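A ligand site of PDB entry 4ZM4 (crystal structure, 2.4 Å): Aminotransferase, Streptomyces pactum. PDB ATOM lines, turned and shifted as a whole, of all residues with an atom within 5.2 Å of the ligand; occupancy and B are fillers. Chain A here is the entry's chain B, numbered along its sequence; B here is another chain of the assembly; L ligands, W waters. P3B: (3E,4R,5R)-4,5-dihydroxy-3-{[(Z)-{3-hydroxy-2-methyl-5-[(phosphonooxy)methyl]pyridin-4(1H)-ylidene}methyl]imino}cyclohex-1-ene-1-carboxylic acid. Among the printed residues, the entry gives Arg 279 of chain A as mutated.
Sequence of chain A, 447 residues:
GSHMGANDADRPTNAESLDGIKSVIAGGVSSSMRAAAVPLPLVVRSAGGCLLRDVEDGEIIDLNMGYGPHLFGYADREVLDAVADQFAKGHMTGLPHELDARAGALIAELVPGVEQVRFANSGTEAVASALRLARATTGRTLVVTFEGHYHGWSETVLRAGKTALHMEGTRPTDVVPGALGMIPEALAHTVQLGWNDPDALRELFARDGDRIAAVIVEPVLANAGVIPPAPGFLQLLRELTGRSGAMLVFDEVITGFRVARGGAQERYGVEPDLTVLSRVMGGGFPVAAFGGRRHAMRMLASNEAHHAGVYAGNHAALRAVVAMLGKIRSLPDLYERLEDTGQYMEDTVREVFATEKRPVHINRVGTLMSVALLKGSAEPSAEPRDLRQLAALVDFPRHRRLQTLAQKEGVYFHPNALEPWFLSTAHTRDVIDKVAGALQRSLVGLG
An oxygen (OAH) of the ligand sits at hydrogen-bond distance from the backbone NH of Thr 124, 3.1 Å away.
OG1 of Thr 124 lies within hydrogen-bond range of OAH of the ligand (2.5 Å).
The side-chain carboxylate of Asp 251 sits at hydrogen-bond distance from a nitrogen (NAP) of the ligand (2.6 Å).
The side-chain amide oxygen of Asn 223 sits at hydrogen-bond distance from an oxygen (OAG) of the ligand (2.6 Å).
An oxygen (OAI) of the ligand sits at hydrogen-bond distance from the backbone NH (N) of Val 310 of chain B, 2.7 Å away.
OG of Ser 31 is in hydrogen-bond range of OAD of the ligand, at 2.7 Å.
N of Gly 309 of chain B sits at hydrogen-bond distance from OAB of the ligand (2.9 Å).
NH2 of Arg 279 is in salt-bridge range of OAI of the ligand.
NE of Arg 34 lies within salt-bridge range of OAD of the ligand.
An oxygen (OAC) of the ligand lies within hydrogen-bond range of the backbone NH (N) of Gly 123 (3.1 Å).
The backbone carbonyl oxygen of Tyr 150 sits close to a nitrogen (NAP) of the ligand (3.3 Å).
Water W1 lies within hydrogen-bond range of OE2 of Glu 125 of chain B (2.6 Å), OAH of the ligand (2.8 Å) and NE1 of Trp 153 (2.9 Å).
Water W3 bridges an oxygen (OAF) of the ligand (3.4 Å) and the side-chain hydroxyl (OH) of Tyr 67 (3.5 Å).
OG1 of Thr 124 lies close to N of Trp 153 (3.2 Å).
The guanidinium group (NH2) of Arg 34 sits at hydrogen-bond distance from the backbone carbonyl oxygen (O) of Val 310 of chain B (3.4 Å).
OG of Ser 31 sits close to N of Met 33 (3.5 Å).
The backbone carbonyl oxygen (O) of Gly 309 of chain B is in hydrogen-bond range of the guanidinium group (NH2) of Arg 34 (2.8 Å).
The backbone NH (N) of Arg 279 is in hydrogen-bond range of the side-chain hydroxyl (OH) of Tyr 311 of chain B.
The side-chain carboxylate (OE2) of Glu 218 is in hydrogen-bond range of the backbone NH (N) of Tyr 150 (2.8 Å).
The side-chain amide oxygen (OD1) of Asn 121 of chain B sits close to the backbone carbonyl oxygen (O) of Tyr 311 of chain B (3.5 Å).
O of Ala 308 of chain B is in hydrogen-bond range of NE1 of Trp 153 (3.3 Å).
Tyr 67 touches the ligand (CD1 to OAF, 3.2 Å).
CB of Ser 122 touches OAC of the ligand, 3.5 Å away.
His 151 touches the ligand (C to CAL, 3.7 Å).
Gly 152 touches the ligand (CA to CAM, 3.5 Å).
Glu 218 touches the ligand.
Val 253 touches the ligand.
Ile 254 touches the ligand.
OE1 of Glu 419 touches OAF of the ligand, at 3.6 Å.
C of Ala 308 of chain B touches OAB of the ligand, 3.998 Å away.
CD2 of Tyr 311 of chain B touches OAC of the ligand, at 3.8 Å.
Hydrophobic or aromatic side chains that line the ligand: Tyr 67, Tyr 150, Val 253, Ile 254, Val 310 of chain B and Tyr 311 of chain B.
20 residues have an atom within 4 Å of the ligand: Ser 31, Arg 34, Tyr 67, Ser 122, Gly 123, Thr 124, Tyr 150, His 151, Gly 152, Glu 218, Asn 223, Asp 251, Val 253, Ile 254, Arg 279, Glu 419, Ala 308 of chain B, Gly 309 of chain B, Val 310 of chain B and Tyr 311 of chain B.
The nearest printed residue that does not touch the ligand is Trp 153 (4.1 Å).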
ATOM      1  N   SER A  31      27.088  -7.092   5.495  1.00  0.00           N
ATOM      2  CA  SER A  31      27.930  -7.458   6.623  1.00  0.00           C
ATOM      3  C   SER A  31      28.804  -8.664   6.248  1.00  0.00           C
ATOM      4  O   SER A  31      28.288  -9.735   5.898  1.00  0.00           O
ATOM      5  CB  SER A  31      27.081  -7.787   7.843  1.00  0.00           C
ATOM      6  OG  SER A  31      27.823  -8.593   8.737  1.00  0.00           O
ATOM      7  N   MET A  33      30.285 -10.945   7.961  1.00  0.00           N
ATOM      8  CA  MET A  33      29.948 -12.214   8.617  1.00  0.00           C
ATOM      9  C   MET A  33      28.705 -12.839   7.992  1.00  0.00           C
ATOM     10  O   MET A  33      28.705 -14.035   7.628  1.00  0.00           O
ATOM     11  CB  MET A  33      29.670 -12.045  10.101  1.00  0.00           C
ATOM     12  CG  MET A  33      30.862 -11.617  10.949  1.00  0.00           C
ATOM     13  SD  MET A  33      30.617  -9.932  11.628  1.00  0.00           S
ATOM     14  CE  MET A  33      31.478  -9.035  10.353  1.00  0.00           C
ATOM     15  N   ARG A  34      27.636 -12.043   7.858  1.00  0.00           N
ATOM     16  CA  ARG A  34      26.364 -12.546   7.370  1.00  0.00           C
ATOM     17  C   ARG A  34      26.375 -12.908   5.871  1.00  0.00           C
ATOM     18  O   ARG A  34      25.435 -13.511   5.367  1.00  0.00           O
ATOM     19  CB  ARG A  34      25.223 -11.562   7.668  1.00  0.00           C
ATOM     20  CG  ARG A  34      24.970 -11.335   9.149  1.00  0.00           C
ATOM     21  CD  ARG A  34      23.720 -10.491   9.397  1.00  0.00           C
ATOM     22  NE  ARG A  34      23.935  -9.067   9.125  1.00  0.00           N
ATOM     23  CZ  ARG A  34      23.344  -8.354   8.166  1.00  0.00           C
ATOM     24  NH1 ARG A  34      22.444  -8.892   7.349  1.00  0.00           N
ATOM     25  NH2 ARG A  34      23.657  -7.070   8.033  1.00  0.00           N
ATOM     26  N   TYR A  67      19.047 -12.551  14.224  1.00  0.00           N
ATOM     27  CA  TYR A  67      20.100 -12.267  15.197  1.00  0.00           C
ATOM     28  C   TYR A  67      19.675 -11.516  16.488  1.00  0.00           C
ATOM     29  O   TYR A  67      20.490 -10.780  17.071  1.00  0.00           O
ATOM     30  CB  TYR A  67      21.290 -11.600  14.489  1.00  0.00           C
ATOM     31  CG  TYR A  67      21.901 -12.413  13.369  1.00  0.00           C
ATOM     32  CD1 TYR A  67      22.887 -13.350  13.608  1.00  0.00           C
ATOM     33  CD2 TYR A  67      21.501 -12.209  12.067  1.00  0.00           C
ATOM     34  CE1 TYR A  67      23.470 -14.070  12.564  1.00  0.00           C
ATOM     35  CE2 TYR A  67      22.098 -12.919  11.021  1.00  0.00           C
ATOM     36  CZ  TYR A  67      23.064 -13.854  11.268  1.00  0.00           C
ATOM     37  OH  TYR A  67      23.625 -14.572  10.219  1.00  0.00           O
ATOM     38  N   SER A 122      22.794   1.794  16.247  1.00  0.00           N
ATOM     39  CA  SER A 122      23.355   0.434  16.263  1.00  0.00           C
ATOM     40  C   SER A 122      24.143   0.142  17.529  1.00  0.00           C
ATOM     41  O   SER A 122      24.570   1.064  18.207  1.00  0.00           O
ATOM     42  CB  SER A 122      24.293   0.285  15.084  1.00  0.00           C
ATOM     43  OG  SER A 122      25.400   1.132  15.255  1.00  0.00           O
ATOM     44  N   GLY A 123      24.309  -1.132  17.856  1.00  0.00           N
ATOM     45  CA  GLY A 123      25.127  -1.516  18.981  1.00  0.00           C
ATOM     46  C   GLY A 123      26.564  -1.031  18.855  1.00  0.00           C
ATOM     47  O   GLY A 123      27.199  -0.661  19.839  1.00  0.00           O
ATOM     48  N   THR A 124      27.069  -1.059  17.641  1.00  0.00           N
ATOM     49  CA  THR A 124      28.393  -0.605  17.372  1.00  0.00           C
ATOM     50  C   THR A 124      28.543   0.860  17.795  1.00  0.00           C
ATOM     51  O   THR A 124      29.539   1.237  18.460  1.00  0.00           O
ATOM     52  CB  THR A 124      28.750  -0.833  15.875  1.00  0.00           C
ATOM     53  OG1 THR A 124      28.932  -2.247  15.645  1.00  0.00           O
ATOM     54  CG2 THR A 124      30.018  -0.091  15.458  1.00  0.00           C
ATOM     55  N   VAL A 127      28.100   1.280  21.708  1.00  0.00           N
ATOM     56  CA  VAL A 127      29.331   0.879  22.377  1.00  0.00           C
ATOM     57  C   VAL A 127      30.415   1.948  22.241  1.00  0.00           C
ATOM     58  O   VAL A 127      31.085   2.308  23.244  1.00  0.00           O
ATOM     59  CB  VAL A 127      29.810  -0.496  21.795  1.00  0.00           C
ATOM     60  CG1 VAL A 127      31.281  -0.785  22.098  1.00  0.00           C
ATOM     61  CG2 VAL A 127      28.930  -1.617  22.328  1.00  0.00           C
ATOM     62  N   TYR A 150      31.894  -9.837  21.671  1.00  0.00           N
ATOM     63  CA  TYR A 150      31.854  -8.958  20.548  1.00  0.00           C
ATOM     64  C   TYR A 150      31.089  -7.684  20.961  1.00  0.00           C
ATOM     65  O   TYR A 150      29.938  -7.755  21.458  1.00  0.00           O
ATOM     66  CB  TYR A 150      31.219  -9.702  19.349  1.00  0.00           C
ATOM     67  CG  TYR A 150      31.087  -8.855  18.088  1.00  0.00           C
ATOM     68  CD1 TYR A 150      32.199  -8.469  17.360  1.00  0.00           C
ATOM     69  CD2 TYR A 150      29.825  -8.476  17.611  1.00  0.00           C
ATOM     70  CE1 TYR A 150      32.068  -7.707  16.211  1.00  0.00           C
ATOM     71  CE2 TYR A 150      29.690  -7.691  16.481  1.00  0.00           C
ATOM     72  CZ  TYR A 150      30.812  -7.311  15.788  1.00  0.00           C
ATOM     73  OH  TYR A 150      30.649  -6.541  14.676  1.00  0.00           O
ATOM     74  N   HIS A 151      31.690  -6.538  20.664  1.00  0.00           N
ATOM     75  CA  HIS A 151      31.090  -5.251  20.975  1.00  0.00           C
ATOM     76  C   HIS A 151      30.940  -4.335  19.764  1.00  0.00           C
ATOM     77  O   HIS A 151      30.902  -3.121  19.878  1.00  0.00           O
ATOM     78  CB  HIS A 151      31.899  -4.625  22.081  1.00  0.00           C
ATOM     79  CG  HIS A 151      32.062  -5.537  23.262  1.00  0.00           C
ATOM     80  ND1 HIS A 151      30.972  -6.078  23.909  1.00  0.00           N
ATOM     81  CD2 HIS A 151      33.160  -6.025  23.875  1.00  0.00           C
ATOM     82  CE1 HIS A 151      31.401  -6.868  24.878  1.00  0.00           C
ATOM     83  NE2 HIS A 151      32.726  -6.853  24.875  1.00  0.00           N
ATOM     84  N   GLY A 152      30.791  -4.923  18.588  1.00  0.00           N
ATOM     85  CA  GLY A 152      30.609  -4.178  17.359  1.00  0.00           C
ATOM     86  C   GLY A 152      31.963  -3.950  16.724  1.00  0.00           C
ATOM     87  O   GLY A 152      32.969  -4.481  17.200  1.00  0.00           O
ATOM     88  N   TRP A 153      31.996  -3.125  15.688  1.00  0.00           N
ATOM     89  CA  TRP A 153      33.177  -3.046  14.830  1.00  0.00           C
ATOM     90  C   TRP A 153      33.873  -1.705  14.892  1.00  0.00           C
ATOM     91  O   TRP A 153      34.661  -1.378  13.992  1.00  0.00           O
ATOM     92  CB  TRP A 153      32.775  -3.378  13.384  1.00  0.00           C
ATOM     93  CG  TRP A 153      31.522  -2.711  12.868  1.00  0.00           C
ATOM     94  CD1 TRP A 153      30.244  -3.086  13.079  1.00  0.00           C
ATOM     95  CD2 TRP A 153      31.460  -1.544  12.052  1.00  0.00           C
ATOM     96  NE1 TRP A 153      29.365  -2.211  12.453  1.00  0.00           N
ATOM     97  CE2 TRP A 153      30.104  -1.280  11.785  1.00  0.00           C
ATOM     98  CE3 TRP A 153      32.431  -0.720  11.472  1.00  0.00           C
ATOM     99  CZ2 TRP A 153      29.697  -0.235  10.980  1.00  0.00           C
ATOM    100  CZ3 TRP A 153      32.037   0.287  10.699  1.00  0.00           C
ATOM    101  CH2 TRP A 153      30.667   0.544  10.448  1.00  0.00           C
ATOM    102  N   GLU A 218      30.034  -9.032  27.676  1.00  0.00           N
ATOM    103  CA  GLU A 218      28.739  -9.680  27.438  1.00  0.00           C
ATOM    104  C   GLU A 218      28.426 -10.474  28.681  1.00  0.00           C
ATOM    105  O   GLU A 218      29.051 -11.500  28.948  1.00  0.00           O
ATOM    106  CB  GLU A 218      28.776 -10.632  26.229  1.00  0.00           C
ATOM    107  CG  GLU A 218      28.863  -9.957  24.872  1.00  0.00           C
ATOM    108  CD  GLU A 218      28.772 -10.959  23.739  1.00  0.00           C
ATOM    109  OE1 GLU A 218      27.827 -11.814  23.748  1.00  0.00           O
ATOM    110  OE2 GLU A 218      29.626 -10.921  22.836  1.00  0.00           O
ATOM    111  N   ASN A 223      27.793 -14.415  21.426  1.00  0.00           N
ATOM    112  CA  ASN A 223      28.433 -14.499  20.100  1.00  0.00           C
ATOM    113  C   ASN A 223      29.560 -15.559  19.977  1.00  0.00           C
ATOM    114  O   ASN A 223      30.401 -15.499  19.073  1.00  0.00           O
ATOM    115  CB  ASN A 223      29.020 -13.131  19.717  1.00  0.00           C
ATOM    116  CG  ASN A 223      27.982 -12.075  19.502  1.00  0.00           C
ATOM    117  OD1 ASN A 223      27.369 -11.974  18.426  1.00  0.00           O
ATOM    118  ND2 ASN A 223      27.819 -11.227  20.478  1.00  0.00           N
ATOM    119  N   ASP A 251      27.477  -5.002  28.009  1.00  0.00           N
ATOM    120  CA  ASP A 251      26.904  -5.013  26.657  1.00  0.00           C
ATOM    121  C   ASP A 251      25.739  -5.957  26.698  1.00  0.00           C
ATOM    122  O   ASP A 251      25.898  -7.154  26.563  1.00  0.00           O
ATOM    123  CB  ASP A 251      27.955  -5.445  25.620  1.00  0.00           C
ATOM    124  CG  ASP A 251      27.467  -5.329  24.208  1.00  0.00           C
ATOM    125  OD1 ASP A 251      26.259  -5.122  23.986  1.00  0.00           O
ATOM    126  OD2 ASP A 251      28.310  -5.476  23.281  1.00  0.00           O
ATOM    127  N   VAL A 253      23.282  -5.859  24.393  1.00  0.00           N
ATOM    128  CA  VAL A 253      22.681  -5.733  23.069  1.00  0.00           C
ATOM    129  C   VAL A 253      21.862  -6.976  22.761  1.00  0.00           C
ATOM    130  O   VAL A 253      20.746  -6.863  22.278  1.00  0.00           O
ATOM    131  CB  VAL A 253      23.772  -5.508  21.970  1.00  0.00           C
ATOM    132  CG1 VAL A 253      23.286  -5.946  20.581  1.00  0.00           C
ATOM    133  CG2 VAL A 253      24.166  -4.037  21.919  1.00  0.00           C
ATOM    134  N   ILE A 254      22.390  -8.131  23.133  1.00  0.00           N
ATOM    135  CA  ILE A 254      21.659  -9.382  22.969  1.00  0.00           C
ATOM    136  C   ILE A 254      20.859  -9.750  24.226  1.00  0.00           C
ATOM    137  O   ILE A 254      19.660 -10.075  24.109  1.00  0.00           O
ATOM    138  CB  ILE A 254      22.615 -10.527  22.572  1.00  0.00           C
ATOM    139  CG1 ILE A 254      22.965 -10.378  21.083  1.00  0.00           C
ATOM    140  CG2 ILE A 254      21.975 -11.882  22.801  1.00  0.00           C
ATOM    141  CD1 ILE A 254      24.055 -11.337  20.642  1.00  0.00           C
ATOM    142  N   SER A 278      20.013  -2.784  22.559  1.00  0.00           N
ATOM    143  CA  SER A 278      19.555  -2.740  21.162  1.00  0.00           C
ATOM    144  C   SER A 278      18.590  -3.922  20.916  1.00  0.00           C
ATOM    145  O   SER A 278      17.988  -4.422  21.851  1.00  0.00           O
ATOM    146  CB  SER A 278      20.732  -2.777  20.190  1.00  0.00           C
ATOM    147  OG  SER A 278      20.350  -2.579  18.851  1.00  0.00           O
ATOM    148  N   ARG A 279      18.428  -4.365  19.686  1.00  0.00           N
ATOM    149  CA  ARG A 279      17.795  -5.666  19.362  1.00  0.00           C
ATOM    150  C   ARG A 279      16.356  -5.793  19.798  1.00  0.00           C
ATOM    151  O   ARG A 279      15.485  -5.316  19.088  1.00  0.00           O
ATOM    152  CB  ARG A 279      18.613  -6.831  19.904  1.00  0.00           C
ATOM    153  CG  ARG A 279      20.036  -6.839  19.430  1.00  0.00           C
ATOM    154  CD  ARG A 279      20.219  -7.335  18.012  1.00  0.00           C
ATOM    155  NE  ARG A 279      21.479  -6.792  17.550  1.00  0.00           N
ATOM    156  CZ  ARG A 279      22.633  -7.451  17.408  1.00  0.00           C
ATOM    157  NH1 ARG A 279      22.761  -8.764  17.657  1.00  0.00           N
ATOM    158  NH2 ARG A 279      23.682  -6.763  16.989  1.00  0.00           N
ATOM    159  N   GLU A 419      27.462 -19.833  16.747  1.00  0.00           N
ATOM    160  CA  GLU A 419      26.442 -18.798  16.605  1.00  0.00           C
ATOM    161  C   GLU A 419      25.104 -19.268  17.185  1.00  0.00           C
ATOM    162  O   GLU A 419      24.569 -20.293  16.795  1.00  0.00           O
ATOM    163  CB  GLU A 419      26.280 -18.431  15.153  1.00  0.00           C
ATOM    164  CG  GLU A 419      27.503 -17.731  14.560  1.00  0.00           C
ATOM    165  CD  GLU A 419      27.707 -16.341  15.124  1.00  0.00           C
ATOM    166  OE1 GLU A 419      26.795 -15.792  15.775  1.00  0.00           O
ATOM    167  OE2 GLU A 419      28.803 -15.797  14.934  1.00  0.00           O
ATOM    168  N   PHE A 422      18.013 -18.021  18.340  1.00  0.00           N
ATOM    169  CA  PHE A 422      17.219 -17.008  19.049  1.00  0.00           C
ATOM    170  C   PHE A 422      15.734 -17.322  18.991  1.00  0.00           C
ATOM    171  O   PHE A 422      15.012 -16.851  18.104  1.00  0.00           O
ATOM    172  CB  PHE A 422      17.465 -15.639  18.402  1.00  0.00           C
ATOM    173  CG  PHE A 422      18.858 -15.117  18.590  1.00  0.00           C
ATOM    174  CD1 PHE A 422      19.827 -15.355  17.657  1.00  0.00           C
ATOM    175  CD2 PHE A 422      19.188 -14.378  19.716  1.00  0.00           C
ATOM    176  CE1 PHE A 422      21.083 -14.827  17.806  1.00  0.00           C
ATOM    177  CE2 PHE A 422      20.463 -13.881  19.876  1.00  0.00           C
ATOM    178  CZ  PHE A 422      21.410 -14.101  18.920  1.00  0.00           C
ATOM    179  N   ASN B 121      23.868   1.703   8.676  1.00  0.00           N
ATOM    180  CA  ASN B 121      22.801   2.427   9.332  1.00  0.00           C
ATOM    181  C   ASN B 121      22.937   3.952   9.303  1.00  0.00           C
ATOM    182  O   ASN B 121      21.965   4.651   9.539  1.00  0.00           O
ATOM    183  CB  ASN B 121      22.673   1.940  10.775  1.00  0.00           C
ATOM    184  CG  ASN B 121      22.487   0.448  10.860  1.00  0.00           C
ATOM    185  OD1 ASN B 121      21.453  -0.076  10.433  1.00  0.00           O
ATOM    186  ND2 ASN B 121      23.490  -0.255  11.410  1.00  0.00           N
ATOM    187  N   GLU B 125      28.927   5.302  10.155  1.00  0.00           N
ATOM    188  CA  GLU B 125      29.303   3.911   9.834  1.00  0.00           C
ATOM    189  C   GLU B 125      29.828   3.739   8.401  1.00  0.00           C
ATOM    190  O   GLU B 125      30.856   3.080   8.191  1.00  0.00           O
ATOM    191  CB  GLU B 125      28.113   2.924  10.062  1.00  0.00           C
ATOM    192  CG  GLU B 125      27.744   2.670  11.517  1.00  0.00           C
ATOM    193  CD  GLU B 125      26.616   1.656  11.657  1.00  0.00           C
ATOM    194  OE1 GLU B 125      25.917   1.371  10.667  1.00  0.00           O
ATOM    195  OE2 GLU B 125      26.441   1.149  12.785  1.00  0.00           O
ATOM    196  N   ALA B 308      30.205  -4.391   8.645  1.00  0.00           N
ATOM    197  CA  ALA B 308      29.341  -5.196   9.486  1.00  0.00           C
ATOM    198  C   ALA B 308      28.195  -4.372  10.013  1.00  0.00           C
ATOM    199  O   ALA B 308      28.015  -3.216   9.632  1.00  0.00           O
ATOM    200  CB  ALA B 308      30.163  -5.809  10.648  1.00  0.00           C
ATOM    201  N   GLY B 309      27.423  -4.986  10.907  1.00  0.00           N
ATOM    202  CA  GLY B 309      26.264  -4.364  11.505  1.00  0.00           C
ATOM    203  C   GLY B 309      25.027  -5.223  11.240  1.00  0.00           C
ATOM    204  O   GLY B 309      24.595  -5.358  10.100  1.00  0.00           O
ATOM    205  N   VAL B 310      24.426  -5.728  12.284  1.00  0.00           N
ATOM    206  CA  VAL B 310      23.280  -6.638  12.146  1.00  0.00           C
ATOM    207  C   VAL B 310      22.119  -6.003  11.383  1.00  0.00           C
ATOM    208  O   VAL B 310      21.452  -6.702  10.639  1.00  0.00           O
ATOM    209  CB  VAL B 310      22.826  -7.146  13.542  1.00  0.00           C
ATOM    210  CG1 VAL B 310      21.874  -6.177  14.205  1.00  0.00           C
ATOM    211  CG2 VAL B 310      22.209  -8.519  13.434  1.00  0.00           C
ATOM    212  N   TYR B 311      21.923  -4.689  11.541  1.00  0.00           N
ATOM    213  CA  TYR B 311      20.826  -3.976  10.869  1.00  0.00           C
ATOM    214  C   TYR B 311      21.211  -3.433   9.460  1.00  0.00           C
ATOM    215  O   TYR B 311      20.353  -2.895   8.762  1.00  0.00           O
ATOM    216  CB  TYR B 311      20.377  -2.764  11.671  1.00  0.00           C
ATOM    217  CG  TYR B 311      19.896  -3.026  13.072  1.00  0.00           C
ATOM    218  CD1 TYR B 311      18.748  -3.793  13.303  1.00  0.00           C
ATOM    219  CD2 TYR B 311      20.540  -2.480  14.161  1.00  0.00           C
ATOM    220  CE1 TYR B 311      18.295  -4.025  14.576  1.00  0.00           C
ATOM    221  CE2 TYR B 311      20.088  -2.712  15.434  1.00  0.00           C
ATOM    222  CZ  TYR B 311      18.978  -3.496  15.635  1.00  0.00           C
ATOM    223  OH  TYR B 311      18.535  -3.725  16.928  1.00  0.00           O
HETATM  224  OAH P3B L   1      26.545  -2.988  15.279  1.00  0.00           O
HETATM  225  PBA P3B L   1      25.304  -3.895  15.687  1.00  0.00           P
HETATM  226  OAI P3B L   1      25.377  -5.030  14.707  1.00  0.00           O
HETATM  227  OAC P3B L   1      23.966  -3.192  15.596  1.00  0.00           O
HETATM  228  OAQ P3B L   1      25.752  -4.395  17.225  1.00  0.00           O
HETATM  229  CAM P3B L   1      27.129  -4.739  17.580  1.00  0.00           C
HETATM  230  CAV P3B L   1      27.056  -5.621  18.620  1.00  0.00           C
HETATM  231  CAL P3B L   1      27.325  -5.121  19.890  1.00  0.00           C
HETATM  232  NAP P3B L   1      27.214  -5.984  20.974  1.00  0.00           N
HETATM  233  CAU P3B L   1      26.827  -7.292  20.809  1.00  0.00           C
HETATM  234  CAA P3B L   1      26.752  -8.140  21.880  1.00  0.00           C
HETATM  235  CAW P3B L   1      26.607  -7.777  19.604  1.00  0.00           C
HETATM  236  OAE P3B L   1      26.233  -9.077  19.515  1.00  0.00           O
HETATM  237  CAX P3B L   1      26.671  -6.981  18.454  1.00  0.00           C
HETATM  238  CAJ P3B L   1      26.423  -7.547  17.162  1.00  0.00           C
HETATM  239  NAO P3B L   1      26.271  -8.899  16.968  1.00  0.00           N
HETATM  240  CAT P3B L   1      26.162  -9.468  15.728  1.00  0.00           C
HETATM  241  CAK P3B L   1      26.350  -8.796  14.484  1.00  0.00           C
HETATM  242  CAS P3B L   1      26.307  -9.411  13.245  1.00  0.00           C
HETATM  243  CAR P3B L   1      26.439  -8.689  12.035  1.00  0.00           C
HETATM  244  OAD P3B L   1      26.292  -9.227  10.931  1.00  0.00           O
HETATM  245  OAB P3B L   1      26.783  -7.535  12.010  1.00  0.00           O
HETATM  246  CAN P3B L   1      25.849 -10.661  13.100  1.00  0.00           C
HETATM  247  CAY P3B L   1      25.471 -11.468  14.357  1.00  0.00           C
HETATM  248  OAF P3B L   1      25.991 -12.778  14.049  1.00  0.00           O
HETATM  249  CAZ P3B L   1      25.991 -10.890  15.746  1.00  0.00           C
HETATM  250  OAG P3B L   1      25.305 -11.366  16.950  1.00  0.00           O
HETATM  251  O   HOH W   1      26.575  -1.415  12.927  1.00  0.00           O
HETATM  252  O   HOH W   2      23.651  -3.023  13.002  1.00  0.00           O
HETATM  253  O   HOH W   3      26.984 -13.992  11.009  1.00  0.00           O
